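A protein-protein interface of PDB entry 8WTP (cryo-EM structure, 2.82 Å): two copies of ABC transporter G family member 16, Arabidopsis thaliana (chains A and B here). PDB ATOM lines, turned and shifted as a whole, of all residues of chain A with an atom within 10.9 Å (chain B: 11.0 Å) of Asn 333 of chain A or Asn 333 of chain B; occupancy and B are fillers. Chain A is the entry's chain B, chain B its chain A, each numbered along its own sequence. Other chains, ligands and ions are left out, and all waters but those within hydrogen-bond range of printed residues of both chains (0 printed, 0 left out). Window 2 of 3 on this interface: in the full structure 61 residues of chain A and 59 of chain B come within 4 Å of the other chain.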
ATOM      1  N   SER A 292      15.159  35.517   0.120  1.00  0.00           N
ATOM      2  CA  SER A 292      15.784  34.290   0.576  1.00  0.00           C
ATOM      3  C   SER A 292      15.386  33.143  -0.349  1.00  0.00           C
ATOM      4  O   SER A 292      14.887  33.349  -1.457  1.00  0.00           O
ATOM      5  CB  SER A 292      15.407  34.004   2.027  1.00  0.00           C
ATOM      6  OG  SER A 292      14.038  33.667   2.141  1.00  0.00           O
ATOM      7  N   HIS A 293      15.611  31.915   0.097  1.00  0.00           N
ATOM      8  CA  HIS A 293      15.297  30.732  -0.689  1.00  0.00           C
ATOM      9  C   HIS A 293      13.948  30.127  -0.334  1.00  0.00           C
ATOM     10  O   HIS A 293      13.242  29.637  -1.219  1.00  0.00           O
ATOM     11  CB  HIS A 293      16.398  29.685  -0.502  1.00  0.00           C
ATOM     12  CG  HIS A 293      16.564  28.761  -1.665  1.00  0.00           C
ATOM     13  ND1 HIS A 293      17.716  28.037  -1.876  1.00  0.00           N
ATOM     14  CD2 HIS A 293      15.725  28.437  -2.676  1.00  0.00           C
ATOM     15  CE1 HIS A 293      17.582  27.311  -2.970  1.00  0.00           C
ATOM     16  NE2 HIS A 293      16.382  27.533  -3.473  1.00  0.00           N
ATOM     17  N   ARG A 294      13.562  30.161   0.937  1.00  0.00           N
ATOM     18  CA  ARG A 294      12.288  29.592   1.350  1.00  0.00           C
ATOM     19  C   ARG A 294      11.127  30.545   1.075  1.00  0.00           C
ATOM     20  O   ARG A 294       9.961  30.143   1.171  1.00  0.00           O
ATOM     21  CB  ARG A 294      12.372  29.209   2.837  1.00  0.00           C
ATOM     22  CG  ARG A 294      11.294  28.257   3.349  1.00  0.00           C
ATOM     23  CD  ARG A 294      11.520  27.859   4.795  1.00  0.00           C
ATOM     24  NE  ARG A 294      11.404  28.991   5.705  1.00  0.00           N
ATOM     25  CZ  ARG A 294      11.651  28.928   7.008  1.00  0.00           C
ATOM     26  NH1 ARG A 294      12.012  27.780   7.563  1.00  0.00           N
ATOM     27  NH2 ARG A 294      11.523  30.010   7.761  1.00  0.00           N
ATOM     28  N   VAL A 295      11.420  31.781   0.673  1.00  0.00           N
ATOM     29  CA  VAL A 295      10.385  32.773   0.412  1.00  0.00           C
ATOM     30  C   VAL A 295       9.818  32.676  -1.004  1.00  0.00           C
ATOM     31  O   VAL A 295       8.696  33.142  -1.244  1.00  0.00           O
ATOM     32  CB  VAL A 295      10.961  34.174   0.703  1.00  0.00           C
ATOM     33  CG1 VAL A 295      11.872  34.629  -0.403  1.00  0.00           C
ATOM     34  CG2 VAL A 295       9.884  35.181   0.954  1.00  0.00           C
ATOM     35  N   LEU A 296      10.525  32.033  -1.932  1.00  0.00           N
ATOM     36  CA  LEU A 296      10.081  31.972  -3.319  1.00  0.00           C
ATOM     37  C   LEU A 296       9.052  30.883  -3.566  1.00  0.00           C
ATOM     38  O   LEU A 296       8.698  30.638  -4.722  1.00  0.00           O
ATOM     39  CB  LEU A 296      11.271  31.771  -4.248  1.00  0.00           C
ATOM     40  CG  LEU A 296      12.322  32.868  -4.168  1.00  0.00           C
ATOM     41  CD1 LEU A 296      13.595  32.379  -4.806  1.00  0.00           C
ATOM     42  CD2 LEU A 296      11.831  34.112  -4.852  1.00  0.00           C
ATOM     43  N   SER A 297       8.571  30.223  -2.518  1.00  0.00           N
ATOM     44  CA  SER A 297       7.347  29.441  -2.586  1.00  0.00           C
ATOM     45  C   SER A 297       6.101  30.315  -2.583  1.00  0.00           C
ATOM     46  O   SER A 297       4.997  29.794  -2.760  1.00  0.00           O
ATOM     47  CB  SER A 297       7.287  28.463  -1.410  1.00  0.00           C
ATOM     48  OG  SER A 297       8.360  27.540  -1.456  1.00  0.00           O
ATOM     49  N   PRO A 320      15.153  29.799 -14.010  1.00  0.00           N
ATOM     50  CA  PRO A 320      16.212  29.007 -14.653  1.00  0.00           C
ATOM     51  C   PRO A 320      16.147  29.006 -16.170  1.00  0.00           C
ATOM     52  O   PRO A 320      17.188  29.165 -16.816  1.00  0.00           O
ATOM     53  CB  PRO A 320      15.990  27.602 -14.084  1.00  0.00           C
ATOM     54  CG  PRO A 320      15.465  27.845 -12.759  1.00  0.00           C
ATOM     55  CD  PRO A 320      14.543  29.010 -12.915  1.00  0.00           C
ATOM     56  N   PRO A 329      23.932  30.100 -17.796  1.00  0.00           N
ATOM     57  CA  PRO A 329      23.114  29.074 -17.132  1.00  0.00           C
ATOM     58  C   PRO A 329      23.187  29.111 -15.614  1.00  0.00           C
ATOM     59  O   PRO A 329      24.056  29.767 -15.030  1.00  0.00           O
ATOM     60  CB  PRO A 329      23.687  27.761 -17.682  1.00  0.00           C
ATOM     61  CG  PRO A 329      24.375  28.147 -18.950  1.00  0.00           C
ATOM     62  CD  PRO A 329      24.941  29.501 -18.683  1.00  0.00           C
ATOM     63  N   ILE A 330      22.270  28.396 -14.972  1.00  0.00           N
ATOM     64  CA  ILE A 330      22.005  28.545 -13.546  1.00  0.00           C
ATOM     65  C   ILE A 330      22.603  27.360 -12.789  1.00  0.00           C
ATOM     66  O   ILE A 330      22.563  26.223 -13.281  1.00  0.00           O
ATOM     67  CB  ILE A 330      20.490  28.703 -13.309  1.00  0.00           C
ATOM     68  CG1 ILE A 330      20.151  28.881 -11.826  1.00  0.00           C
ATOM     69  CG2 ILE A 330      19.701  27.568 -13.960  1.00  0.00           C
ATOM     70  CD1 ILE A 330      18.777  29.456 -11.585  1.00  0.00           C
ATOM     71  N   PRO A 331      23.219  27.579 -11.624  1.00  0.00           N
ATOM     72  CA  PRO A 331      23.665  26.443 -10.808  1.00  0.00           C
ATOM     73  C   PRO A 331      22.544  25.899  -9.944  1.00  0.00           C
ATOM     74  O   PRO A 331      21.879  26.655  -9.232  1.00  0.00           O
ATOM     75  CB  PRO A 331      24.794  27.036  -9.953  1.00  0.00           C
ATOM     76  CG  PRO A 331      25.039  28.418 -10.496  1.00  0.00           C
ATOM     77  CD  PRO A 331      23.763  28.848 -11.122  1.00  0.00           C
ATOM     78  N   GLU A 332      22.324  24.591 -10.000  1.00  0.00           N
ATOM     79  CA  GLU A 332      21.262  23.953  -9.237  1.00  0.00           C
ATOM     80  C   GLU A 332      21.694  23.745  -7.790  1.00  0.00           C
ATOM     81  O   GLU A 332      22.876  23.840  -7.455  1.00  0.00           O
ATOM     82  CB  GLU A 332      20.868  22.622  -9.880  1.00  0.00           C
ATOM     83  CG  GLU A 332      20.169  22.756 -11.226  1.00  0.00           C
ATOM     84  CD  GLU A 332      21.131  22.899 -12.392  1.00  0.00           C
ATOM     85  OE1 GLU A 332      22.359  22.821 -12.174  1.00  0.00           O
ATOM     86  OE2 GLU A 332      20.656  23.097 -13.529  1.00  0.00           O
ATOM     87  N   ASN A 333      20.703  23.438  -6.941  1.00  0.00           N
ATOM     88  CA  ASN A 333      20.857  23.305  -5.485  1.00  0.00           C
ATOM     89  C   ASN A 333      21.499  24.551  -4.880  1.00  0.00           C
ATOM     90  O   ASN A 333      22.389  24.477  -4.032  1.00  0.00           O
ATOM     91  CB  ASN A 333      21.635  22.037  -5.113  1.00  0.00           C
ATOM     92  CG  ASN A 333      20.729  20.842  -4.893  1.00  0.00           C
ATOM     93  OD1 ASN A 333      19.665  20.961  -4.293  1.00  0.00           O
ATOM     94  ND2 ASN A 333      21.146  19.683  -5.386  1.00  0.00           N
ATOM     95  N   GLU A 334      21.027  25.708  -5.331  1.00  0.00           N
ATOM     96  CA  GLU A 334      21.636  26.991  -5.030  1.00  0.00           C
ATOM     97  C   GLU A 334      20.534  28.032  -5.127  1.00  0.00           C
ATOM     98  O   GLU A 334      19.545  27.841  -5.839  1.00  0.00           O
ATOM     99  CB  GLU A 334      22.801  27.277  -5.994  1.00  0.00           C
ATOM    100  CG  GLU A 334      23.730  28.433  -5.631  1.00  0.00           C
ATOM    101  CD  GLU A 334      23.287  29.755  -6.226  1.00  0.00           C
ATOM    102  OE1 GLU A 334      22.625  29.736  -7.285  1.00  0.00           O
ATOM    103  OE2 GLU A 334      23.610  30.810  -5.641  1.00  0.00           O
ATOM    104  N   ASN A 335      20.694  29.122  -4.378  1.00  0.00           N
ATOM    105  CA  ASN A 335      19.615  30.089  -4.224  1.00  0.00           C
ATOM    106  C   ASN A 335      19.389  30.856  -5.516  1.00  0.00           C
ATOM    107  O   ASN A 335      20.242  31.638  -5.948  1.00  0.00           O
ATOM    108  CB  ASN A 335      19.920  31.055  -3.085  1.00  0.00           C
ATOM    109  CG  ASN A 335      18.785  32.025  -2.830  1.00  0.00           C
ATOM    110  OD1 ASN A 335      17.614  31.690  -3.012  1.00  0.00           O
ATOM    111  ND2 ASN A 335      19.120  33.226  -2.386  1.00  0.00           N
ATOM    112  N   GLN A 336      18.229  30.628  -6.124  1.00  0.00           N
ATOM    113  CA  GLN A 336      17.739  31.410  -7.243  1.00  0.00           C
ATOM    114  C   GLN A 336      17.385  32.814  -6.764  1.00  0.00           C
ATOM    115  O   GLN A 336      17.332  33.090  -5.560  1.00  0.00           O
ATOM    116  CB  GLN A 336      16.519  30.727  -7.851  1.00  0.00           C
ATOM    117  CG  GLN A 336      16.813  29.343  -8.385  1.00  0.00           C
ATOM    118  CD  GLN A 336      15.561  28.585  -8.756  1.00  0.00           C
ATOM    119  OE1 GLN A 336      14.446  29.056  -8.531  1.00  0.00           O
ATOM    120  NE2 GLN A 336      15.735  27.400  -9.317  1.00  0.00           N
ATOM    121  N   THR A 337      17.196  33.725  -7.727  1.00  0.00           N
ATOM    122  CA  THR A 337      16.819  35.133  -7.553  1.00  0.00           C
ATOM    123  C   THR A 337      17.889  35.943  -6.794  1.00  0.00           C
ATOM    124  O   THR A 337      17.691  37.129  -6.501  1.00  0.00           O
ATOM    125  CB  THR A 337      15.434  35.249  -6.879  1.00  0.00           C
ATOM    126  OG1 THR A 337      15.495  34.594  -5.611  1.00  0.00           O
ATOM    127  CG2 THR A 337      14.380  34.486  -7.638  1.00  0.00           C
ATOM    128  N   GLU A 338      19.031  35.341  -6.500  1.00  0.00           N
ATOM    129  CA  GLU A 338      20.268  35.886  -5.959  1.00  0.00           C
ATOM    130  C   GLU A 338      21.406  35.729  -6.946  1.00  0.00           C
ATOM    131  O   GLU A 338      22.144  36.690  -7.180  1.00  0.00           O
ATOM    132  CB  GLU A 338      20.624  35.186  -4.641  1.00  0.00           C
ATOM    133  CG  GLU A 338      22.025  35.471  -4.124  1.00  0.00           C
ATOM    134  CD  GLU A 338      22.126  35.393  -2.609  1.00  0.00           C
ATOM    135  OE1 GLU A 338      21.486  34.500  -2.014  1.00  0.00           O
ATOM    136  OE2 GLU A 338      22.860  36.213  -2.015  1.00  0.00           O
ATOM    137  N   PHE A 339      21.566  34.532  -7.518  1.00  0.00           N
ATOM    138  CA  PHE A 339      22.415  34.344  -8.687  1.00  0.00           C
ATOM    139  C   PHE A 339      21.946  35.214  -9.843  1.00  0.00           C
ATOM    140  O   PHE A 339      22.760  35.811 -10.552  1.00  0.00           O
ATOM    141  CB  PHE A 339      22.418  32.862  -9.085  1.00  0.00           C
ATOM    142  CG  PHE A 339      22.588  32.625 -10.563  1.00  0.00           C
ATOM    143  CD1 PHE A 339      23.837  32.736 -11.156  1.00  0.00           C
ATOM    144  CD2 PHE A 339      21.499  32.285 -11.359  1.00  0.00           C
ATOM    145  CE1 PHE A 339      23.989  32.530 -12.511  1.00  0.00           C
ATOM    146  CE2 PHE A 339      21.651  32.085 -12.713  1.00  0.00           C
ATOM    147  CZ  PHE A 339      22.896  32.202 -13.287  1.00  0.00           C
ATOM    148  N   SER B 292      23.837  32.431   4.686  1.00  0.00           N
ATOM    149  CA  SER B 292      23.156  32.282   3.410  1.00  0.00           C
ATOM    150  C   SER B 292      23.462  30.914   2.806  1.00  0.00           C
ATOM    151  O   SER B 292      23.922  29.994   3.485  1.00  0.00           O
ATOM    152  CB  SER B 292      23.547  33.414   2.464  1.00  0.00           C
ATOM    153  OG  SER B 292      24.898  33.299   2.066  1.00  0.00           O
ATOM    154  N   HIS B 293      23.189  30.765   1.515  1.00  0.00           N
ATOM    155  CA  HIS B 293      23.404  29.512   0.807  1.00  0.00           C
ATOM    156  C   HIS B 293      24.733  29.467   0.067  1.00  0.00           C
ATOM    157  O   HIS B 293      25.364  28.410   0.003  1.00  0.00           O
ATOM    158  CB  HIS B 293      22.259  29.277  -0.181  1.00  0.00           C
ATOM    159  CG  HIS B 293      21.971  27.834  -0.445  1.00  0.00           C
ATOM    160  ND1 HIS B 293      20.727  27.384  -0.826  1.00  0.00           N
ATOM    161  CD2 HIS B 293      22.766  26.740  -0.391  1.00  0.00           C
ATOM    162  CE1 HIS B 293      20.765  26.074  -0.987  1.00  0.00           C
ATOM    163  NE2 HIS B 293      21.992  25.660  -0.732  1.00  0.00           N
ATOM    164  N   ARG B 294      25.182  30.589  -0.489  1.00  0.00           N
ATOM    165  CA  ARG B 294      26.449  30.611  -1.206  1.00  0.00           C
ATOM    166  C   ARG B 294      27.648  30.706  -0.271  1.00  0.00           C
ATOM    167  O   ARG B 294      28.791  30.616  -0.734  1.00  0.00           O
ATOM    168  CB  ARG B 294      26.465  31.776  -2.200  1.00  0.00           C
ATOM    169  CG  ARG B 294      27.270  31.513  -3.459  1.00  0.00           C
ATOM    170  CD  ARG B 294      27.113  32.630  -4.466  1.00  0.00           C
ATOM    171  NE  ARG B 294      27.061  33.936  -3.823  1.00  0.00           N
ATOM    172  CZ  ARG B 294      27.326  35.081  -4.440  1.00  0.00           C
ATOM    173  NH1 ARG B 294      27.678  35.082  -5.718  1.00  0.00           N
ATOM    174  NH2 ARG B 294      27.248  36.224  -3.777  1.00  0.00           N
ATOM    175  N   VAL B 295      27.413  30.866   1.033  1.00  0.00           N
ATOM    176  CA  VAL B 295      28.486  31.004   2.010  1.00  0.00           C
ATOM    177  C   VAL B 295      28.958  29.661   2.554  1.00  0.00           C
ATOM    178  O   VAL B 295      30.086  29.569   3.060  1.00  0.00           O
ATOM    179  CB  VAL B 295      27.989  31.952   3.122  1.00  0.00           C
ATOM    180  CG1 VAL B 295      27.007  31.256   4.010  1.00  0.00           C
ATOM    181  CG2 VAL B 295      29.118  32.524   3.923  1.00  0.00           C
ATOM    182  N   LEU B 296      28.162  28.600   2.416  1.00  0.00           N
ATOM    183  CA  LEU B 296      28.526  27.297   2.957  1.00  0.00           C
ATOM    184  C   LEU B 296      29.474  26.525   2.055  1.00  0.00           C
ATOM    185  O   LEU B 296      29.773  25.364   2.346  1.00  0.00           O
ATOM    186  CB  LEU B 296      27.276  26.465   3.219  1.00  0.00           C
ATOM    187  CG  LEU B 296      26.280  27.093   4.183  1.00  0.00           C
ATOM    188  CD1 LEU B 296      24.950  26.398   4.043  1.00  0.00           C
ATOM    189  CD2 LEU B 296      26.782  26.987   5.593  1.00  0.00           C
ATOM    190  N   SER B 297      29.944  27.134   0.974  1.00  0.00           N
ATOM    191  CA  SER B 297      31.122  26.669   0.259  1.00  0.00           C
ATOM    192  C   SER B 297      32.413  27.029   0.980  1.00  0.00           C
ATOM    193  O   SER B 297      33.490  26.620   0.536  1.00  0.00           O
ATOM    194  CB  SER B 297      31.144  27.262  -1.153  1.00  0.00           C
ATOM    195  OG  SER B 297      30.017  26.842  -1.903  1.00  0.00           O
ATOM    196  N   PRO B 320      23.019  17.278   6.135  1.00  0.00           N
ATOM    197  CA  PRO B 320      21.887  16.420   5.750  1.00  0.00           C
ATOM    198  C   PRO B 320      21.885  15.062   6.427  1.00  0.00           C
ATOM    199  O   PRO B 320      20.821  14.609   6.865  1.00  0.00           O
ATOM    200  CB  PRO B 320      22.057  16.283   4.233  1.00  0.00           C
ATOM    201  CG  PRO B 320      22.647  17.542   3.838  1.00  0.00           C
ATOM    202  CD  PRO B 320      23.631  17.860   4.917  1.00  0.00           C
ATOM    203  N   PRO B 329      14.152  14.569   8.389  1.00  0.00           N
ATOM    204  CA  PRO B 329      14.936  14.655   7.152  1.00  0.00           C
ATOM    205  C   PRO B 329      14.891  16.041   6.526  1.00  0.00           C
ATOM    206  O   PRO B 329      14.069  16.894   6.867  1.00  0.00           O
ATOM    207  CB  PRO B 329      14.275  13.618   6.238  1.00  0.00           C
ATOM    208  CG  PRO B 329      13.558  12.698   7.168  1.00  0.00           C
ATOM    209  CD  PRO B 329      13.081  13.568   8.283  1.00  0.00           C
ATOM    210  N   ILE B 330      15.805  16.245   5.587  1.00  0.00           N
ATOM    211  CA  ILE B 330      16.105  17.567   5.053  1.00  0.00           C
ATOM    212  C   ILE B 330      15.489  17.711   3.664  1.00  0.00           C
ATOM    213  O   ILE B 330      15.532  16.766   2.862  1.00  0.00           O
ATOM    214  CB  ILE B 330      17.626  17.803   5.060  1.00  0.00           C
ATOM    215  CG1 ILE B 330      17.995  19.168   4.474  1.00  0.00           C
ATOM    216  CG2 ILE B 330      18.369  16.647   4.392  1.00  0.00           C
ATOM    217  CD1 ILE B 330      19.397  19.601   4.810  1.00  0.00           C
ATOM    218  N   PRO B 331      14.855  18.842   3.351  1.00  0.00           N
ATOM    219  CA  PRO B 331      14.358  19.055   1.986  1.00  0.00           C
ATOM    220  C   PRO B 331      15.479  19.537   1.077  1.00  0.00           C
ATOM    221  O   PRO B 331      16.224  20.455   1.423  1.00  0.00           O
ATOM    222  CB  PRO B 331      13.280  20.133   2.160  1.00  0.00           C
ATOM    223  CG  PRO B 331      13.050  20.238   3.643  1.00  0.00           C
ATOM    224  CD  PRO B 331      14.345  19.864   4.274  1.00  0.00           C
ATOM    225  N   GLU B 332      15.595  18.909  -0.088  1.00  0.00           N
ATOM    226  CA  GLU B 332      16.574  19.318  -1.080  1.00  0.00           C
ATOM    227  C   GLU B 332      16.054  20.512  -1.871  1.00  0.00           C
ATOM    228  O   GLU B 332      14.880  20.879  -1.775  1.00  0.00           O
ATOM    229  CB  GLU B 332      16.915  18.152  -2.008  1.00  0.00           C
ATOM    230  CG  GLU B 332      17.735  17.051  -1.348  1.00  0.00           C
ATOM    231  CD  GLU B 332      16.896  16.052  -0.568  1.00  0.00           C
ATOM    232  OE1 GLU B 332      15.651  16.145  -0.606  1.00  0.00           O
ATOM    233  OE2 GLU B 332      17.491  15.176   0.094  1.00  0.00           O
ATOM    234  N   ASN B 333      16.959  21.110  -2.663  1.00  0.00           N
ATOM    235  CA  ASN B 333      16.731  22.371  -3.388  1.00  0.00           C
ATOM    236  C   ASN B 333      16.278  23.478  -2.438  1.00  0.00           C
ATOM    237  O   ASN B 333      15.391  24.275  -2.751  1.00  0.00           O
ATOM    238  CB  ASN B 333      15.738  22.200  -4.546  1.00  0.00           C
ATOM    239  CG  ASN B 333      16.361  21.541  -5.762  1.00  0.00           C
ATOM    240  OD1 ASN B 333      17.489  21.856  -6.143  1.00  0.00           O
ATOM    241  ND2 ASN B 333      15.627  20.625  -6.378  1.00  0.00           N
ATOM    242  N   GLU B 334      16.898  23.521  -1.264  1.00  0.00           N
ATOM    243  CA  GLU B 334      16.461  24.373  -0.173  1.00  0.00           C
ATOM    244  C   GLU B 334      17.663  24.599   0.730  1.00  0.00           C
ATOM    245  O   GLU B 334      18.561  23.756   0.804  1.00  0.00           O
ATOM    246  CB  GLU B 334      15.285  23.728   0.578  1.00  0.00           C
ATOM    247  CG  GLU B 334      14.499  24.639   1.515  1.00  0.00           C
ATOM    248  CD  GLU B 334      15.046  24.648   2.925  1.00  0.00           C
ATOM    249  OE1 GLU B 334      15.650  23.635   3.335  1.00  0.00           O
ATOM    250  OE2 GLU B 334      14.861  25.666   3.625  1.00  0.00           O
ATOM    251  N   ASN B 335      17.680  25.749   1.396  1.00  0.00           N
ATOM    252  CA  ASN B 335      18.873  26.186   2.107  1.00  0.00           C
ATOM    253  C   ASN B 335      19.077  25.367   3.372  1.00  0.00           C
ATOM    254  O   ASN B 335      18.264  25.427   4.300  1.00  0.00           O
ATOM    255  CB  ASN B 335      18.775  27.666   2.455  1.00  0.00           C
ATOM    256  CG  ASN B 335      20.058  28.201   3.050  1.00  0.00           C
ATOM    257  OD1 ASN B 335      21.148  27.756   2.699  1.00  0.00           O
ATOM    258  ND2 ASN B 335      19.937  29.162   3.955  1.00  0.00           N
ATOM    259  N   GLN B 336      20.168  24.607   3.407  1.00  0.00           N
ATOM    260  CA  GLN B 336      20.631  24.006   4.644  1.00  0.00           C
ATOM    261  C   GLN B 336      21.188  25.093   5.556  1.00  0.00           C
ATOM    262  O   GLN B 336      21.388  26.241   5.144  1.00  0.00           O
ATOM    263  CB  GLN B 336      21.694  22.954   4.361  1.00  0.00           C
ATOM    264  CG  GLN B 336      21.449  22.183   3.085  1.00  0.00           C
ATOM    265  CD  GLN B 336      22.717  21.605   2.507  1.00  0.00           C
ATOM    266  OE1 GLN B 336      23.819  22.046   2.832  1.00  0.00           O
ATOM    267  NE2 GLN B 336      22.570  20.611   1.646  1.00  0.00           N
ATOM    268  N   THR B 337      21.387  24.731   6.828  1.00  0.00           N
ATOM    269  CA  THR B 337      21.844  25.583   7.932  1.00  0.00           C
ATOM    270  C   THR B 337      20.864  26.734   8.231  1.00  0.00           C
ATOM    271  O   THR B 337      21.172  27.629   9.027  1.00  0.00           O
ATOM    272  CB  THR B 337      23.269  26.116   7.676  1.00  0.00           C
ATOM    273  OG1 THR B 337      23.265  26.863   6.457  1.00  0.00           O
ATOM    274  CG2 THR B 337      24.237  24.989   7.425  1.00  0.00           C
ATOM    275  N   GLU B 338      19.687  26.723   7.613  1.00  0.00           N
ATOM    276  CA  GLU B 338      18.527  27.544   7.922  1.00  0.00           C
ATOM    277  C   GLU B 338      17.331  26.691   8.286  1.00  0.00           C
ATOM    278  O   GLU B 338      16.642  26.985   9.266  1.00  0.00           O
ATOM    279  CB  GLU B 338      18.173  28.429   6.720  1.00  0.00           C
ATOM    280  CG  GLU B 338      16.832  29.141   6.814  1.00  0.00           C
ATOM    281  CD  GLU B 338      16.801  30.449   6.045  1.00  0.00           C
ATOM    282  OE1 GLU B 338      17.521  30.557   5.029  1.00  0.00           O
ATOM    283  OE2 GLU B 338      16.054  31.365   6.450  1.00  0.00           O
ATOM    284  N   PHE B 339      17.086  25.628   7.512  1.00  0.00           N
ATOM    285  CA  PHE B 339      16.160  24.579   7.920  1.00  0.00           C
ATOM    286  C   PHE B 339      16.618  23.932   9.216  1.00  0.00           C
ATOM    287  O   PHE B 339      15.822  23.740  10.140  1.00  0.00           O
ATOM    288  CB  PHE B 339      16.038  23.534   6.805  1.00  0.00           C
ATOM    289  CG  PHE B 339      15.766  22.135   7.301  1.00  0.00           C
ATOM    290  CD1 PHE B 339      14.497  21.769   7.730  1.00  0.00           C
ATOM    291  CD2 PHE B 339      16.777  21.180   7.329  1.00  0.00           C
ATOM    292  CE1 PHE B 339      14.252  20.493   8.196  1.00  0.00           C
ATOM    293  CE2 PHE B 339      16.535  19.907   7.799  1.00  0.00           C
ATOM    294  CZ  PHE B 339      15.273  19.561   8.226  1.00  0.00           C
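OD1 of Asn 333 of chain B lies close to OD1 of Asn 333 of chain A, at 3.0 Å. The backbone carbonyl oxygen of Asn 333 of chain B lies within hydrogen-bond range of a ring nitrogen (NE2) of His 293 of chain A (3.5 Å). ND1 of His 293 of chain A lies within hydrogen-bond range of ND1 of His 293 of chain B.
OE1 of Glu 338 of chain B lies within hydrogen-bond range of ND2 of Asn 335 of chain B (3.0 Å). The side-chain amide nitrogen of Asn 335 of chain A lies within hydrogen-bond range of the side-chain carboxylate of Glu 338 of chain A.
His 293 of chain A touches Asn 335 of chain B (ND1 to N, 3.99 Å). Asn 333 of chain A touches His 293 of chain B (O to NE2, 3.5 Å). N of Asn 335 of chain A touches ND1 of His 293 of chain B, at 3.95 Å.
Printed residues of chain B within 4 Å of His 293 of chain A: His 293 (3.3 Å), Asn 333 (3.5 Å) and Asn 335 (3.99 Å). No residue of chain B comes within 4 Å of Glu 332 of chain A. Asn 333 of chain A touches just these residues of chain B: His 293 (3.5 Å) and Asn 333 (3.0 Å). No residue of chain B comes within 4 Å of Glu 334 of chain A. Of the printed residues of chain A, His 293 of chain B touches His 293 (3.3 Å), Asn 333 (3.5 Å) and Asn 335 (3.95 Å). No residue of chain A comes within 4 Å of Glu 332 of chain B.
Of the 18 printed residues of chain B, 3 touch a printed residue of chain A. Hydrophobic or aromatic side chains of chain B within 4 Å of the printed part of chain A: His 293. Printed residues of chain A that touch a printed residue of chain B: His 293, Asn 333 and Asn 335. Hydrophobic or aromatic side chains of chain A that line the printed part of chain B: His 293. Along chain A the printed residues that touch a printed residue of chain B span positions 293 to 335. Among the printed residues, no Asp or Glu carboxylate lies within 4 Å of a Lys or Arg side-chain nitrogen of the other chain.
His 293 of chain A touches its own counterpart, His 293 of chain B. His 293 of chain A touches Asn 333 of chain B, and with the chains exchanged Asn 333 of chain A touches His 293 of chain B. His 293 of chain A touches Asn 335 of chain B, and with the chains exchanged Asn 335 of chain A touches His 293 of chain B. Asn 333 of chain A touches its own counterpart, Asn 333 of chain B. Of the 6 pairs that touch across the chains among the printed residues, 6 have their exchanged pair printed and touching as well.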
